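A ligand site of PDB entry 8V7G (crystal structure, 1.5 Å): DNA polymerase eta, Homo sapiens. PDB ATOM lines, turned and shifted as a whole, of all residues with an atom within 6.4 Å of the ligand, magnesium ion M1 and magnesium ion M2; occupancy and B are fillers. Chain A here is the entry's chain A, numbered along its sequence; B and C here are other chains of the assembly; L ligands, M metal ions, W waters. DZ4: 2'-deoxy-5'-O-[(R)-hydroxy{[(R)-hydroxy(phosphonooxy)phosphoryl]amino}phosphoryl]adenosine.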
ATOM      1  N   ASP A  16       0.669  10.635 -14.615  1.00  0.00           N
ATOM      2  CA  ASP A  16       1.324  10.788 -15.915  1.00  0.00           C
ATOM      3  C   ASP A  16       0.819   9.746 -16.896  1.00  0.00           C
ATOM      4  O   ASP A  16       0.930   8.544 -16.644  1.00  0.00           O
ATOM      5  CB  ASP A  16       2.852  10.717 -15.777  1.00  0.00           C
ATOM      6  CG  ASP A  16       3.559  11.125 -17.040  1.00  0.00           C
ATOM      7  OD1 ASP A  16       3.457  10.359 -18.007  1.00  0.00           O
ATOM      8  OD2 ASP A  16       4.135  12.228 -17.114  1.00  0.00           O
ATOM      9  N   MET A  17       0.363  10.221 -18.052  1.00  0.00           N
ATOM     10  CA  MET A  17      -0.241   9.301 -18.999  1.00  0.00           C
ATOM     11  C   MET A  17       0.856   8.416 -19.585  1.00  0.00           C
ATOM     12  O   MET A  17       1.985   8.857 -19.825  1.00  0.00           O
ATOM     13  CB  MET A  17      -0.970  10.092 -20.115  1.00  0.00           C
ATOM     14  CG  MET A  17      -2.031  11.046 -19.539  1.00  0.00           C
ATOM     15  SD  MET A  17      -3.290  10.298 -18.493  1.00  0.00           S
ATOM     16  CE  MET A  17      -4.099   9.120 -19.517  1.00  0.00           C
ATOM     17  N   ASP A  18       0.535   7.139 -19.785  1.00  0.00           N
ATOM     18  CA  ASP A  18       1.481   6.233 -20.433  1.00  0.00           C
ATOM     19  C   ASP A  18       1.531   6.487 -21.931  1.00  0.00           C
ATOM     20  O   ASP A  18       0.486   6.645 -22.567  1.00  0.00           O
ATOM     21  CB  ASP A  18       1.130   4.768 -20.155  1.00  0.00           C
ATOM     22  CG  ASP A  18       1.134   4.426 -18.668  1.00  0.00           C
ATOM     23  OD1 ASP A  18       1.867   5.062 -17.895  1.00  0.00           O
ATOM     24  OD2 ASP A  18       0.402   3.507 -18.279  1.00  0.00           O
ATOM     25  N   CYS A  19       2.748   6.574 -22.484  1.00  0.00           N
ATOM     26  CA  CYS A  19       3.015   6.795 -23.915  1.00  0.00           C
ATOM     27  C   CYS A  19       1.887   7.594 -24.560  1.00  0.00           C
ATOM     28  O   CYS A  19       1.197   7.104 -25.475  1.00  0.00           O
ATOM     29  CB  CYS A  19       3.279   5.468 -24.646  1.00  0.00           C
ATOM     30  SG  CYS A  19       2.104   4.126 -24.503  1.00  0.00           S
ATOM     31  N   PHE A  20       1.681   8.826 -24.098  1.00  0.00           N
ATOM     32  CA  PHE A  20       0.374   9.491 -24.250  1.00  0.00           C
ATOM     33  C   PHE A  20      -0.047   9.658 -25.707  1.00  0.00           C
ATOM     34  O   PHE A  20      -1.149   9.238 -26.083  1.00  0.00           O
ATOM     35  CB  PHE A  20       0.397  10.849 -23.547  1.00  0.00           C
ATOM     36  CG  PHE A  20      -0.909  11.566 -23.614  1.00  0.00           C
ATOM     37  CD1 PHE A  20      -2.114  10.902 -23.301  1.00  0.00           C
ATOM     38  CD2 PHE A  20      -0.968  12.908 -23.973  1.00  0.00           C
ATOM     39  CE1 PHE A  20      -3.342  11.575 -23.359  1.00  0.00           C
ATOM     40  CE2 PHE A  20      -2.209  13.590 -24.012  1.00  0.00           C
ATOM     41  CZ  PHE A  20      -3.379  12.922 -23.711  1.00  0.00           C
ATOM     42  N   PHE A  21       0.789  10.280 -26.542  1.00  0.00           N
ATOM     43  CA  PHE A  21       0.338  10.506 -27.932  1.00  0.00           C
ATOM     44  C   PHE A  21       0.070   9.188 -28.644  1.00  0.00           C
ATOM     45  O   PHE A  21      -0.835   9.102 -29.487  1.00  0.00           O
ATOM     46  CB  PHE A  21       1.357  11.324 -28.732  1.00  0.00           C
ATOM     47  CG  PHE A  21       1.485  12.768 -28.338  1.00  0.00           C
ATOM     48  CD1 PHE A  21       0.986  13.268 -27.140  1.00  0.00           C
ATOM     49  CD2 PHE A  21       2.190  13.641 -29.168  1.00  0.00           C
ATOM     50  CE1 PHE A  21       1.146  14.636 -26.798  1.00  0.00           C
ATOM     51  CE2 PHE A  21       2.355  14.981 -28.821  1.00  0.00           C
ATOM     52  CZ  PHE A  21       1.832  15.480 -27.643  1.00  0.00           C
ATOM     53  N   VAL A  22       0.848   8.143 -28.344  1.00  0.00           N
ATOM     54  CA  VAL A  22       0.561   6.830 -28.903  1.00  0.00           C
ATOM     55  C   VAL A  22      -0.829   6.343 -28.470  1.00  0.00           C
ATOM     56  O   VAL A  22      -1.609   5.857 -29.293  1.00  0.00           O
ATOM     57  CB  VAL A  22       1.647   5.825 -28.496  1.00  0.00           C
ATOM     58  CG1 VAL A  22       1.183   4.389 -28.797  1.00  0.00           C
ATOM     59  CG2 VAL A  22       2.971   6.140 -29.199  1.00  0.00           C
ATOM     60  N   GLN A  41       6.646  13.128 -36.240  1.00  0.00           N
ATOM     61  CA  GLN A  41       6.412  14.464 -36.788  1.00  0.00           C
ATOM     62  C   GLN A  41       7.187  14.601 -38.081  1.00  0.00           C
ATOM     63  O   GLN A  41       8.400  14.370 -38.097  1.00  0.00           O
ATOM     64  CB  GLN A  41       6.848  15.579 -35.829  1.00  0.00           C
ATOM     65  CG  GLN A  41       5.853  15.925 -34.767  1.00  0.00           C
ATOM     66  CD  GLN A  41       6.289  17.095 -33.901  1.00  0.00           C
ATOM     67  OE1 GLN A  41       5.447  17.882 -33.460  1.00  0.00           O
ATOM     68  NE2 GLN A  41       7.587  17.220 -33.655  1.00  0.00           N
ATOM     69  N   ILE A  51       8.287  11.199 -31.460  1.00  0.00           N
ATOM     70  CA  ILE A  51       8.030  11.925 -30.228  1.00  0.00           C
ATOM     71  C   ILE A  51       7.332  11.102 -29.150  1.00  0.00           C
ATOM     72  O   ILE A  51       7.283  11.553 -27.999  1.00  0.00           O
ATOM     73  CB  ILE A  51       7.261  13.237 -30.477  1.00  0.00           C
ATOM     74  CG1 ILE A  51       5.912  12.996 -31.162  1.00  0.00           C
ATOM     75  CG2 ILE A  51       8.151  14.217 -31.271  1.00  0.00           C
ATOM     76  CD1 ILE A  51       5.052  14.261 -31.201  1.00  0.00           C
ATOM     77  N   ALA A  52       6.833   9.900 -29.460  1.00  0.00           N
ATOM     78  CA  ALA A  52       6.210   9.023 -28.460  1.00  0.00           C
ATOM     79  C   ALA A  52       6.305   7.588 -28.943  1.00  0.00           C
ATOM     80  O   ALA A  52       6.253   7.337 -30.146  1.00  0.00           O
ATOM     81  CB  ALA A  52       4.739   9.394 -28.195  1.00  0.00           C
ATOM     82  N   VAL A  53       6.462   6.639 -27.996  1.00  0.00           N
ATOM     83  CA  VAL A  53       6.803   5.249 -28.291  1.00  0.00           C
ATOM     84  C   VAL A  53       6.009   4.318 -27.391  1.00  0.00           C
ATOM     85  O   VAL A  53       6.056   4.450 -26.161  1.00  0.00           O
ATOM     86  CB  VAL A  53       8.306   5.005 -28.082  1.00  0.00           C
ATOM     87  CG1 VAL A  53       8.665   3.615 -28.543  1.00  0.00           C
ATOM     88  CG2 VAL A  53       9.131   5.997 -28.844  1.00  0.00           C
ATOM     89  N   TYR A  55       5.110   0.848 -25.384  1.00  0.00           N
ATOM     90  CA  TYR A  55       6.018   0.030 -24.584  1.00  0.00           C
ATOM     91  C   TYR A  55       6.489  -1.207 -25.354  1.00  0.00           C
ATOM     92  O   TYR A  55       7.654  -1.625 -25.213  1.00  0.00           O
ATOM     93  CB  TYR A  55       5.357  -0.311 -23.235  1.00  0.00           C
ATOM     94  CG  TYR A  55       5.445   0.868 -22.269  1.00  0.00           C
ATOM     95  CD1 TYR A  55       4.562   1.959 -22.366  1.00  0.00           C
ATOM     96  CD2 TYR A  55       6.476   0.950 -21.327  1.00  0.00           C
ATOM     97  CE1 TYR A  55       4.679   3.069 -21.516  1.00  0.00           C
ATOM     98  CE2 TYR A  55       6.602   2.040 -20.477  1.00  0.00           C
ATOM     99  CZ  TYR A  55       5.712   3.098 -20.583  1.00  0.00           C
ATOM    100  OH  TYR A  55       5.875   4.179 -19.732  1.00  0.00           O
ATOM    101  N   ARG A  58       9.322   0.103 -27.274  1.00  0.00           N
ATOM    102  CA  ARG A  58      10.477   0.365 -26.400  1.00  0.00           C
ATOM    103  C   ARG A  58      11.288  -0.910 -26.142  1.00  0.00           C
ATOM    104  O   ARG A  58      12.513  -0.830 -25.995  1.00  0.00           O
ATOM    105  CB  ARG A  58      10.024   0.976 -25.078  1.00  0.00           C
ATOM    106  CG  ARG A  58       9.411   2.373 -25.199  1.00  0.00           C
ATOM    107  CD  ARG A  58       8.964   2.875 -23.847  1.00  0.00           C
ATOM    108  NE  ARG A  58       7.977   3.946 -24.002  1.00  0.00           N
ATOM    109  CZ  ARG A  58       7.677   4.851 -23.088  1.00  0.00           C
ATOM    110  NH1 ARG A  58       8.247   4.838 -21.891  1.00  0.00           N
ATOM    111  NH2 ARG A  58       6.743   5.770 -23.350  1.00  0.00           N
ATOM    112  N   ARG A  64      12.151   8.143 -28.125  1.00  0.00           N
ATOM    113  CA  ARG A  64      11.873   9.503 -28.624  1.00  0.00           C
ATOM    114  C   ARG A  64      13.170  10.127 -29.146  1.00  0.00           C
ATOM    115  O   ARG A  64      14.235   9.715 -28.664  1.00  0.00           O
ATOM    116  CB  ARG A  64      11.294  10.339 -27.469  1.00  0.00           C
ATOM    117  CG  ARG A  64      11.147  11.822 -27.744  1.00  0.00           C
ATOM    118  CD  ARG A  64      10.696  12.493 -26.454  1.00  0.00           C
ATOM    119  NE  ARG A  64      11.693  12.364 -25.407  1.00  0.00           N
ATOM    120  CZ  ARG A  64      11.464  11.875 -24.190  1.00  0.00           C
ATOM    121  NH1 ARG A  64      10.255  11.486 -23.844  1.00  0.00           N
ATOM    122  NH2 ARG A  64      12.454  11.784 -23.317  1.00  0.00           N
ATOM    123  N   LEU A  92      -0.650  20.222 -32.916  1.00  0.00           N
ATOM    124  CA  LEU A  92      -0.796  19.315 -31.771  1.00  0.00           C
ATOM    125  C   LEU A  92      -2.220  19.329 -31.174  1.00  0.00           C
ATOM    126  O   LEU A  92      -2.414  18.816 -30.065  1.00  0.00           O
ATOM    127  CB  LEU A  92       0.247  19.664 -30.703  1.00  0.00           C
ATOM    128  CG  LEU A  92       1.710  19.687 -31.186  1.00  0.00           C
ATOM    129  CD1 LEU A  92       2.652  20.172 -30.085  1.00  0.00           C
ATOM    130  CD2 LEU A  92       2.105  18.288 -31.646  1.00  0.00           C
ATOM    131  N   SER A 116       2.249  19.220 -17.430  1.00  0.00           N
ATOM    132  CA  SER A 116       2.589  19.111 -18.850  1.00  0.00           C
ATOM    133  C   SER A 116       1.329  18.686 -19.582  1.00  0.00           C
ATOM    134  O   SER A 116       0.298  18.420 -18.970  1.00  0.00           O
ATOM    135  CB  SER A 116       3.725  18.114 -19.111  1.00  0.00           C
ATOM    136  OG  SER A 116       3.241  16.774 -19.093  1.00  0.00           O
ATOM    137  N   ILE A 117       1.461  18.505 -20.904  1.00  0.00           N
ATOM    138  CA  ILE A 117       0.319  18.058 -21.691  1.00  0.00           C
ATOM    139  C   ILE A 117      -0.249  16.732 -21.168  1.00  0.00           C
ATOM    140  O   ILE A 117      -1.434  16.445 -21.358  1.00  0.00           O
ATOM    141  CB  ILE A 117       0.701  17.963 -23.185  1.00  0.00           C
ATOM    142  CG1 ILE A 117      -0.558  17.899 -24.042  1.00  0.00           C
ATOM    143  CG2 ILE A 117       1.595  16.754 -23.444  1.00  0.00           C
ATOM    144  CD1 ILE A 117      -0.313  18.218 -25.513  1.00  0.00           C
ATOM    145  N   ASP A 118       0.571  15.886 -20.512  1.00  0.00           N
ATOM    146  CA  ASP A 118       0.054  14.597 -20.064  1.00  0.00           C
ATOM    147  C   ASP A 118       0.207  14.353 -18.564  1.00  0.00           C
ATOM    148  O   ASP A 118       0.067  13.193 -18.127  1.00  0.00           O
ATOM    149  CB  ASP A 118       0.674  13.449 -20.869  1.00  0.00           C
ATOM    150  CG  ASP A 118       1.946  12.892 -20.252  1.00  0.00           C
ATOM    151  OD1 ASP A 118       2.756  13.666 -19.694  1.00  0.00           O
ATOM    152  OD2 ASP A 118       2.140  11.642 -20.315  1.00  0.00           O
ATOM    153  N   GLU A 119       0.429  15.377 -17.752  1.00  0.00           N
ATOM    154  CA  GLU A 119       0.562  15.057 -16.329  1.00  0.00           C
ATOM    155  C   GLU A 119       0.096  16.202 -15.470  1.00  0.00           C
ATOM    156  O   GLU A 119       0.206  17.383 -15.853  1.00  0.00           O
ATOM    157  CB  GLU A 119       1.986  14.737 -15.885  1.00  0.00           C
ATOM    158  CG  GLU A 119       2.953  15.811 -16.227  1.00  0.00           C
ATOM    159  CD  GLU A 119       4.372  15.324 -16.302  1.00  0.00           C
ATOM    160  OE1 GLU A 119       5.035  15.036 -15.280  1.00  0.00           O
ATOM    161  OE2 GLU A 119       4.754  15.070 -17.453  1.00  0.00           O
ATOM    162  N   SER A 216       0.088   6.083 -15.222  1.00  0.00           N
ATOM    163  CA  SER A 216       0.761   5.700 -13.986  1.00  0.00           C
ATOM    164  C   SER A 216       0.699   6.864 -13.021  1.00  0.00           C
ATOM    165  O   SER A 216       0.364   7.979 -13.388  1.00  0.00           O
ATOM    166  CB  SER A 216       2.205   5.274 -14.253  1.00  0.00           C
ATOM    167  OG  SER A 216       2.220   4.197 -15.185  1.00  0.00           O
ATOM    168  N   LYS A 227       6.504  12.658  -8.302  1.00  0.00           N
ATOM    169  CA  LYS A 227       6.979  12.514  -9.670  1.00  0.00           C
ATOM    170  C   LYS A 227       7.986  11.367  -9.776  1.00  0.00           C
ATOM    171  O   LYS A 227       7.895  10.532 -10.693  1.00  0.00           O
ATOM    172  CB  LYS A 227       7.596  13.833 -10.163  1.00  0.00           C
ATOM    173  CG  LYS A 227       8.299  13.729 -11.507  1.00  0.00           C
ATOM    174  CD  LYS A 227       7.308  13.452 -12.624  1.00  0.00           C
ATOM    175  CE  LYS A 227       8.001  13.456 -13.969  1.00  0.00           C
ATOM    176  NZ  LYS A 227       7.057  13.171 -15.093  1.00  0.00           N
ATOM    177  N   LYS A 234       6.047   2.353 -14.081  1.00  0.00           N
ATOM    178  CA  LYS A 234       5.362   2.492 -15.361  1.00  0.00           C
ATOM    179  C   LYS A 234       5.533   1.219 -16.193  1.00  0.00           C
ATOM    180  O   LYS A 234       6.601   0.594 -16.173  1.00  0.00           O
ATOM    181  CB  LYS A 234       5.968   3.662 -16.119  1.00  0.00           C
ATOM    182  CG  LYS A 234       5.390   5.007 -15.789  1.00  0.00           C
ATOM    183  CD  LYS A 234       5.689   6.047 -16.857  1.00  0.00           C
ATOM    184  CE  LYS A 234       4.753   7.283 -16.691  1.00  0.00           C
ATOM    185  NZ  LYS A 234       3.536   7.277 -17.585  1.00  0.00           N
ATOM    186  N   PRO A 235       4.538   0.840 -17.007  1.00  0.00           N
ATOM    187  CA  PRO A 235       3.248   1.532 -17.218  1.00  0.00           C
ATOM    188  C   PRO A 235       2.105   0.928 -16.418  1.00  0.00           C
ATOM    189  O   PRO A 235       2.179  -0.194 -15.881  1.00  0.00           O
ATOM    190  CB  PRO A 235       2.998   1.325 -18.711  1.00  0.00           C
ATOM    191  CG  PRO A 235       3.550  -0.062 -18.970  1.00  0.00           C
ATOM    192  CD  PRO A 235       4.753  -0.189 -18.037  1.00  0.00           C
ATOM    193  P   U7B B   8      10.286  14.973 -17.636  1.00  0.00           P
ATOM    194  C5' U7B B   8       7.837  15.979 -18.113  1.00  0.00           C
ATOM    195  O5' U7B B   8       8.999  15.311 -18.609  1.00  0.00           O
ATOM    196  C4' U7B B   8       7.167  16.611 -19.236  1.00  0.00           C
ATOM    197  O4' U7B B   8       8.126  17.411 -19.962  1.00  0.00           O
ATOM    198  C3' U7B B   8       6.745  15.575 -20.282  1.00  0.00           C
ATOM    199  O3' U7B B   8       5.421  15.049 -19.987  1.00  0.00           O
ATOM    200  C2' U7B B   8       6.686  16.418 -21.588  1.00  0.00           C
ATOM    201  C1' U7B B   8       7.614  17.684 -21.256  1.00  0.00           C
ATOM    202  N1  U7B B   8       8.731  17.896 -22.133  1.00  0.00           N
ATOM    203  C2  U7B B   8       8.529  18.540 -23.336  1.00  0.00           C
ATOM    204  O2  U7B B   8       7.400  18.869 -23.668  1.00  0.00           O
ATOM    205  N3  U7B B   8       9.582  18.808 -24.144  1.00  0.00           N
ATOM    206  C4  U7B B   8      10.809  18.453 -23.799  1.00  0.00           C
ATOM    207  N4  U7B B   8      11.815  18.719 -24.611  1.00  0.00           N
ATOM    208  C5  U7B B   8      11.037  17.795 -22.573  1.00  0.00           C
ATOM    209  C6  U7B B   8      10.000  17.540 -21.755  1.00  0.00           C
ATOM    210  OP1 U7B B   8       9.833  14.080 -16.513  1.00  0.00           O
ATOM    211  OP2 U7B B   8      11.381  14.362 -18.458  1.00  0.00           O
ATOM    212  F1  U7B B   8       5.421  16.867 -21.793  1.00  0.00           F
ATOM    213  F2  U7B B   8       7.071  15.727 -22.669  1.00  0.00           F
ATOM    214  P    DT C   4      14.952  20.007 -35.853  1.00  0.00           P
ATOM    215  OP1  DT C   4      14.726  20.160 -37.308  1.00  0.00           O
ATOM    216  OP2  DT C   4      15.681  21.061 -35.103  1.00  0.00           O
ATOM    217  O5'  DT C   4      13.538  19.784 -35.163  1.00  0.00           O
ATOM    218  C5'  DT C   4      12.597  18.901 -35.732  1.00  0.00           C
ATOM    219  C4'  DT C   4      11.220  19.183 -35.176  1.00  0.00           C
ATOM    220  O4'  DT C   4      11.094  18.610 -33.868  1.00  0.00           O
ATOM    221  C3'  DT C   4      10.867  20.661 -35.015  1.00  0.00           C
ATOM    222  O3'  DT C   4       9.551  20.812 -35.436  1.00  0.00           O
ATOM    223  C2'  DT C   4      11.040  20.917 -33.506  1.00  0.00           C
ATOM    224  C1'  DT C   4      10.611  19.568 -32.951  1.00  0.00           C
ATOM    225  N1   DT C   4      11.171  19.218 -31.641  1.00  0.00           N
ATOM    226  C2   DT C   4      10.361  18.540 -30.783  1.00  0.00           C
ATOM    227  O2   DT C   4       9.195  18.272 -31.043  1.00  0.00           O
ATOM    228  N3   DT C   4      10.933  18.196 -29.600  1.00  0.00           N
ATOM    229  C4   DT C   4      12.228  18.426 -29.191  1.00  0.00           C
ATOM    230  O4   DT C   4      12.642  18.055 -28.102  1.00  0.00           O
ATOM    231  C5   DT C   4      13.060  19.125 -30.150  1.00  0.00           C
ATOM    232  C7   DT C   4      14.485  19.441 -29.813  1.00  0.00           C
ATOM    233  C6   DT C   4      12.492  19.484 -31.328  1.00  0.00           C
ATOM    234  P    DG C   5       8.837  22.243 -35.455  1.00  0.00           P
ATOM    235  OP1  DG C   5       8.006  22.314 -36.670  1.00  0.00           O
ATOM    236  OP2  DG C   5       9.855  23.275 -35.194  1.00  0.00           O
ATOM    237  O5'  DG C   5       7.888  22.173 -34.170  1.00  0.00           O
ATOM    238  C5'  DG C   5       6.789  21.278 -34.145  1.00  0.00           C
ATOM    239  C4'  DG C   5       6.054  21.427 -32.842  1.00  0.00           C
ATOM    240  O4'  DG C   5       6.895  20.938 -31.761  1.00  0.00           O
ATOM    241  C3'  DG C   5       5.701  22.874 -32.467  1.00  0.00           C
ATOM    242  O3'  DG C   5       4.439  22.879 -31.819  1.00  0.00           O
ATOM    243  C2'  DG C   5       6.819  23.251 -31.500  1.00  0.00           C
ATOM    244  C1'  DG C   5       6.963  21.938 -30.764  1.00  0.00           C
ATOM    245  N9   DG C   5       8.190  21.790 -30.035  1.00  0.00           N
ATOM    246  C8   DG C   5       9.437  22.283 -30.365  1.00  0.00           C
ATOM    247  N7   DG C   5      10.366  21.980 -29.483  1.00  0.00           N
ATOM    248  C5   DG C   5       9.673  21.253 -28.516  1.00  0.00           C
ATOM    249  C6   DG C   5      10.130  20.665 -27.301  1.00  0.00           C
ATOM    250  O6   DG C   5      11.275  20.658 -26.824  1.00  0.00           O
ATOM    251  N1   DG C   5       9.099  20.019 -26.622  1.00  0.00           N
ATOM    252  C2   DG C   5       7.808  19.961 -27.048  1.00  0.00           C
ATOM    253  N2   DG C   5       6.952  19.298 -26.263  1.00  0.00           N
ATOM    254  N3   DG C   5       7.361  20.504 -28.167  1.00  0.00           N
ATOM    255  C4   DG C   5       8.359  21.131 -28.842  1.00  0.00           C
HETATM  256  N1  DZ4 L   1       9.176  16.848 -27.950  1.00  0.00           N
HETATM  257  C2  DZ4 L   1       7.901  16.842 -28.353  1.00  0.00           C
HETATM  258  N3  DZ4 L   1       6.930  16.164 -27.772  1.00  0.00           N
HETATM  259  C4  DZ4 L   1       7.279  15.448 -26.681  1.00  0.00           C
HETATM  260  C5  DZ4 L   1       8.593  15.402 -26.202  1.00  0.00           C
HETATM  261  C6  DZ4 L   1       9.558  16.142 -26.873  1.00  0.00           C
HETATM  262  N6  DZ4 L   1      10.844  16.148 -26.479  1.00  0.00           N
HETATM  263  N7  DZ4 L   1       8.599  14.596 -25.111  1.00  0.00           N
HETATM  264  C8  DZ4 L   1       7.335  14.146 -24.923  1.00  0.00           C
HETATM  265  N9  DZ4 L   1       6.542  14.659 -25.880  1.00  0.00           N
HETATM  266  PA  DZ4 L   1       6.014  11.972 -21.507  1.00  0.00           P
HETATM  267  PB  DZ4 L   1       4.982   9.495 -22.732  1.00  0.00           P
HETATM  268  PG  DZ4 L   1       5.629   7.661 -20.553  1.00  0.00           P
HETATM  269  C1' DZ4 L   1       5.082  14.429 -26.013  1.00  0.00           C
HETATM  270  O1A DZ4 L   1       5.120  11.819 -20.352  1.00  0.00           O
HETATM  271  O1B DZ4 L   1       3.716   9.878 -22.084  1.00  0.00           O
HETATM  272  O1G DZ4 L   1       5.070   8.791 -19.735  1.00  0.00           O
HETATM  273  C2' DZ4 L   1       4.711  13.031 -26.497  1.00  0.00           C
HETATM  274  O2A DZ4 L   1       7.472  12.462 -21.160  1.00  0.00           O
HETATM  275  O2B DZ4 L   1       4.939   9.266 -24.243  1.00  0.00           O
HETATM  276  O2G DZ4 L   1       4.794   6.383 -20.425  1.00  0.00           O
HETATM  277  C3' DZ4 L   1       4.453  12.284 -25.191  1.00  0.00           C
HETATM  278  O3' DZ4 L   1       3.509  11.235 -25.412  1.00  0.00           O
HETATM  279  N3A DZ4 L   1       6.176  10.558 -22.341  1.00  0.00           N
HETATM  280  O3B DZ4 L   1       5.489   8.111 -22.126  1.00  0.00           O
HETATM  281  O3G DZ4 L   1       7.136   7.350 -20.351  1.00  0.00           O
HETATM  282  C4' DZ4 L   1       3.823  13.393 -24.353  1.00  0.00           C
HETATM  283  O4' DZ4 L   1       4.486  14.623 -24.736  1.00  0.00           O
HETATM  284  C5' DZ4 L   1       4.040  13.157 -22.827  1.00  0.00           C
HETATM  285  O5' DZ4 L   1       5.430  13.073 -22.532  1.00  0.00           O
HETATM  286 MG    MG M   1       3.578  10.248 -20.009  1.00  0.00          MG
HETATM  287 MG    MG M   2       4.710  13.387 -18.794  1.00  0.00          MG
HETATM  288  O   HOH W   1       8.819   6.046 -18.666  1.00  0.00           O
HETATM  289  O   HOH W   2       7.903  10.811 -24.948  1.00  0.00           O
HETATM  290  O   HOH W   3       4.973  17.427 -24.351  1.00  0.00           O
HETATM  291  O   HOH W   4       6.801   7.727 -25.421  1.00  0.00           O
HETATM  292  O   HOH W   5       9.535  14.081 -22.452  1.00  0.00           O
HETATM  293  O   HOH W   6       6.739  12.875 -18.211  1.00  0.00           O
HETATM  294  O   HOH W   7       4.668  17.475 -28.777  1.00  0.00           O
HETATM  295  O   HOH W   8       9.112   8.348 -21.734  1.00  0.00           O
HETATM  296  O   HOH W   9       6.773  10.076 -17.906  1.00  0.00           O
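N4 of U7B 8 of chain B sits at hydrogen-bond distance from N6 of the ligand (3.3 Å).
The side-chain hydroxyl (OH) of Tyr 55 is in hydrogen-bond range of an oxygen (O2G) of the ligand (2.6 Å).
O4 of DT 4 of chain C lies within hydrogen-bond range of a nitrogen (N6) of the ligand.
The backbone NH of Cys 19 is in hydrogen-bond range of an oxygen (O2G) of the ligand, at 2.9 Å.
The guanidinium group of Arg 58 is in salt-bridge range of an oxygen (O3G) of the ligand, 3.1 Å away.
An oxygen (O2G) of the ligand is in salt-bridge range of the side-chain amino group (NZ) of Lys 234, 3.2 Å away.
The backbone NH (N) of Phe 20 lies within hydrogen-bond range of an oxygen (O2B) of the ligand (3.3 Å).
The backbone NH (N) of Phe 21 sits at hydrogen-bond distance from an oxygen (O3') of the ligand (3.1 Å).
NH1 of Arg 64 lies within salt-bridge range of O2A of the ligand (3.99 Å).
NZ of Lys 234 sits at hydrogen-bond distance from O of Asp 16 (3.0 Å).
The backbone NH of Asp 16 lies within hydrogen-bond range of the backbone carbonyl oxygen of Ser 216, at 2.9 Å.
O of Met 17 sits close to NZ of Lys 234 (3.1 Å).
The backbone NH (N) of Glu 119 lies close to the side-chain hydroxyl (OG) of Ser 116, 3.4 Å away.
O3' of U7B 8 of chain B sits close to OG of Ser 116 (2.9 Å).
OP1 of U7B 8 of chain B lies within salt-bridge range of the side-chain amino group (NZ) of Lys 227.
NE2 of Gln 41 lies within hydrogen-bond range of O2 of DT 4 of chain C, 3.2 Å away.
O of Val 53 sits at hydrogen-bond distance from NE of Arg 58 (2.9 Å).
N1 of DG 5 of chain C sits close to a nitrogen (N1) of the ligand, at 3.4 Å.
Residues that only touch the ligand: Asp 18 (3.3 Å), Ile 51 (3.3 Å), Ala 52 (3.6 Å) and Ile 117 (3.8 Å).
Hydrophobic or aromatic side chains that line the ligand: Phe 20, Phe 21, Ile 51, Ala 52, Tyr 55 and Ile 117.
Of the 26 residues printed, 17 come within 4 Å of the ligand.
Residues that only touch magnesium ion M1: Lys 234.
Within 4 Å of magnesium ion M1: Asp 16, Met 17, Asp 118 and Lys 234.
The nearest printed residue that does not touch magnesium ion M1 is Asp 18 (4.4 Å).
Residues that only touch magnesium ion M2: Ser 116.
Within 4 Å of magnesium ion M2: Asp 16, Ser 116, Asp 118, Glu 119 and U7B 8 of chain B.
OD1 of Asp 16 binds magnesium ion M1, 2.0 Å away.
Magnesium ion M1 is bound by the side-chain carboxylate (OD2) of Asp 118, 2.0 Å away.
O1G of the ligand binds magnesium ion M1 (2.1 Å).
Magnesium ion M1 is bound by O1B of the ligand (2.1 Å).
Magnesium ion M1 is bound by O of Met 17, at 2.1 Å.
Magnesium ion M1 is bound by an oxygen (O1A) of the ligand (2.2 Å).
Magnesium ion M1 has six donor atoms within binding distance.
Magnesium ion M2 is bound by the side-chain carboxylate (OD2) of Asp 16 (2.1 Å).
OE2 of Glu 119 binds magnesium ion M2.
Magnesium ion M2 is bound by O3' of U7B 8 of chain B (2.2 Å).
OD1 of Asp 118 binds magnesium ion M2.
Water W6 binds magnesium ion M2 (2.2 Å).
Magnesium ion M2 is bound by O1A of the ligand (2.2 Å).
Water W6 lies within hydrogen-bond range of O2A of the ligand (3.1 Å), NZ of Lys 227 (3.1 Å) and O5' of U7B 8 of chain B (3.3 Å).
Water W4 lies within hydrogen-bond range of O2B of the ligand (2.7 Å), N of Val 53 (2.8 Å) and NH2 of Arg 58 (2.8 Å).
Water W1 bridges O3G of the ligand and NH1 of Arg 58.
Water W5 lies within hydrogen-bond range of a nitrogen (N7) of the ligand (2.9 Å) and the guanidinium group of Arg 64 (3.0 Å).
Water W2 lies within hydrogen-bond range of NH1 of Arg 64 (2.7 Å), N3A of the ligand (3.1 Å) and O of Ile 51 (3.2 Å).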
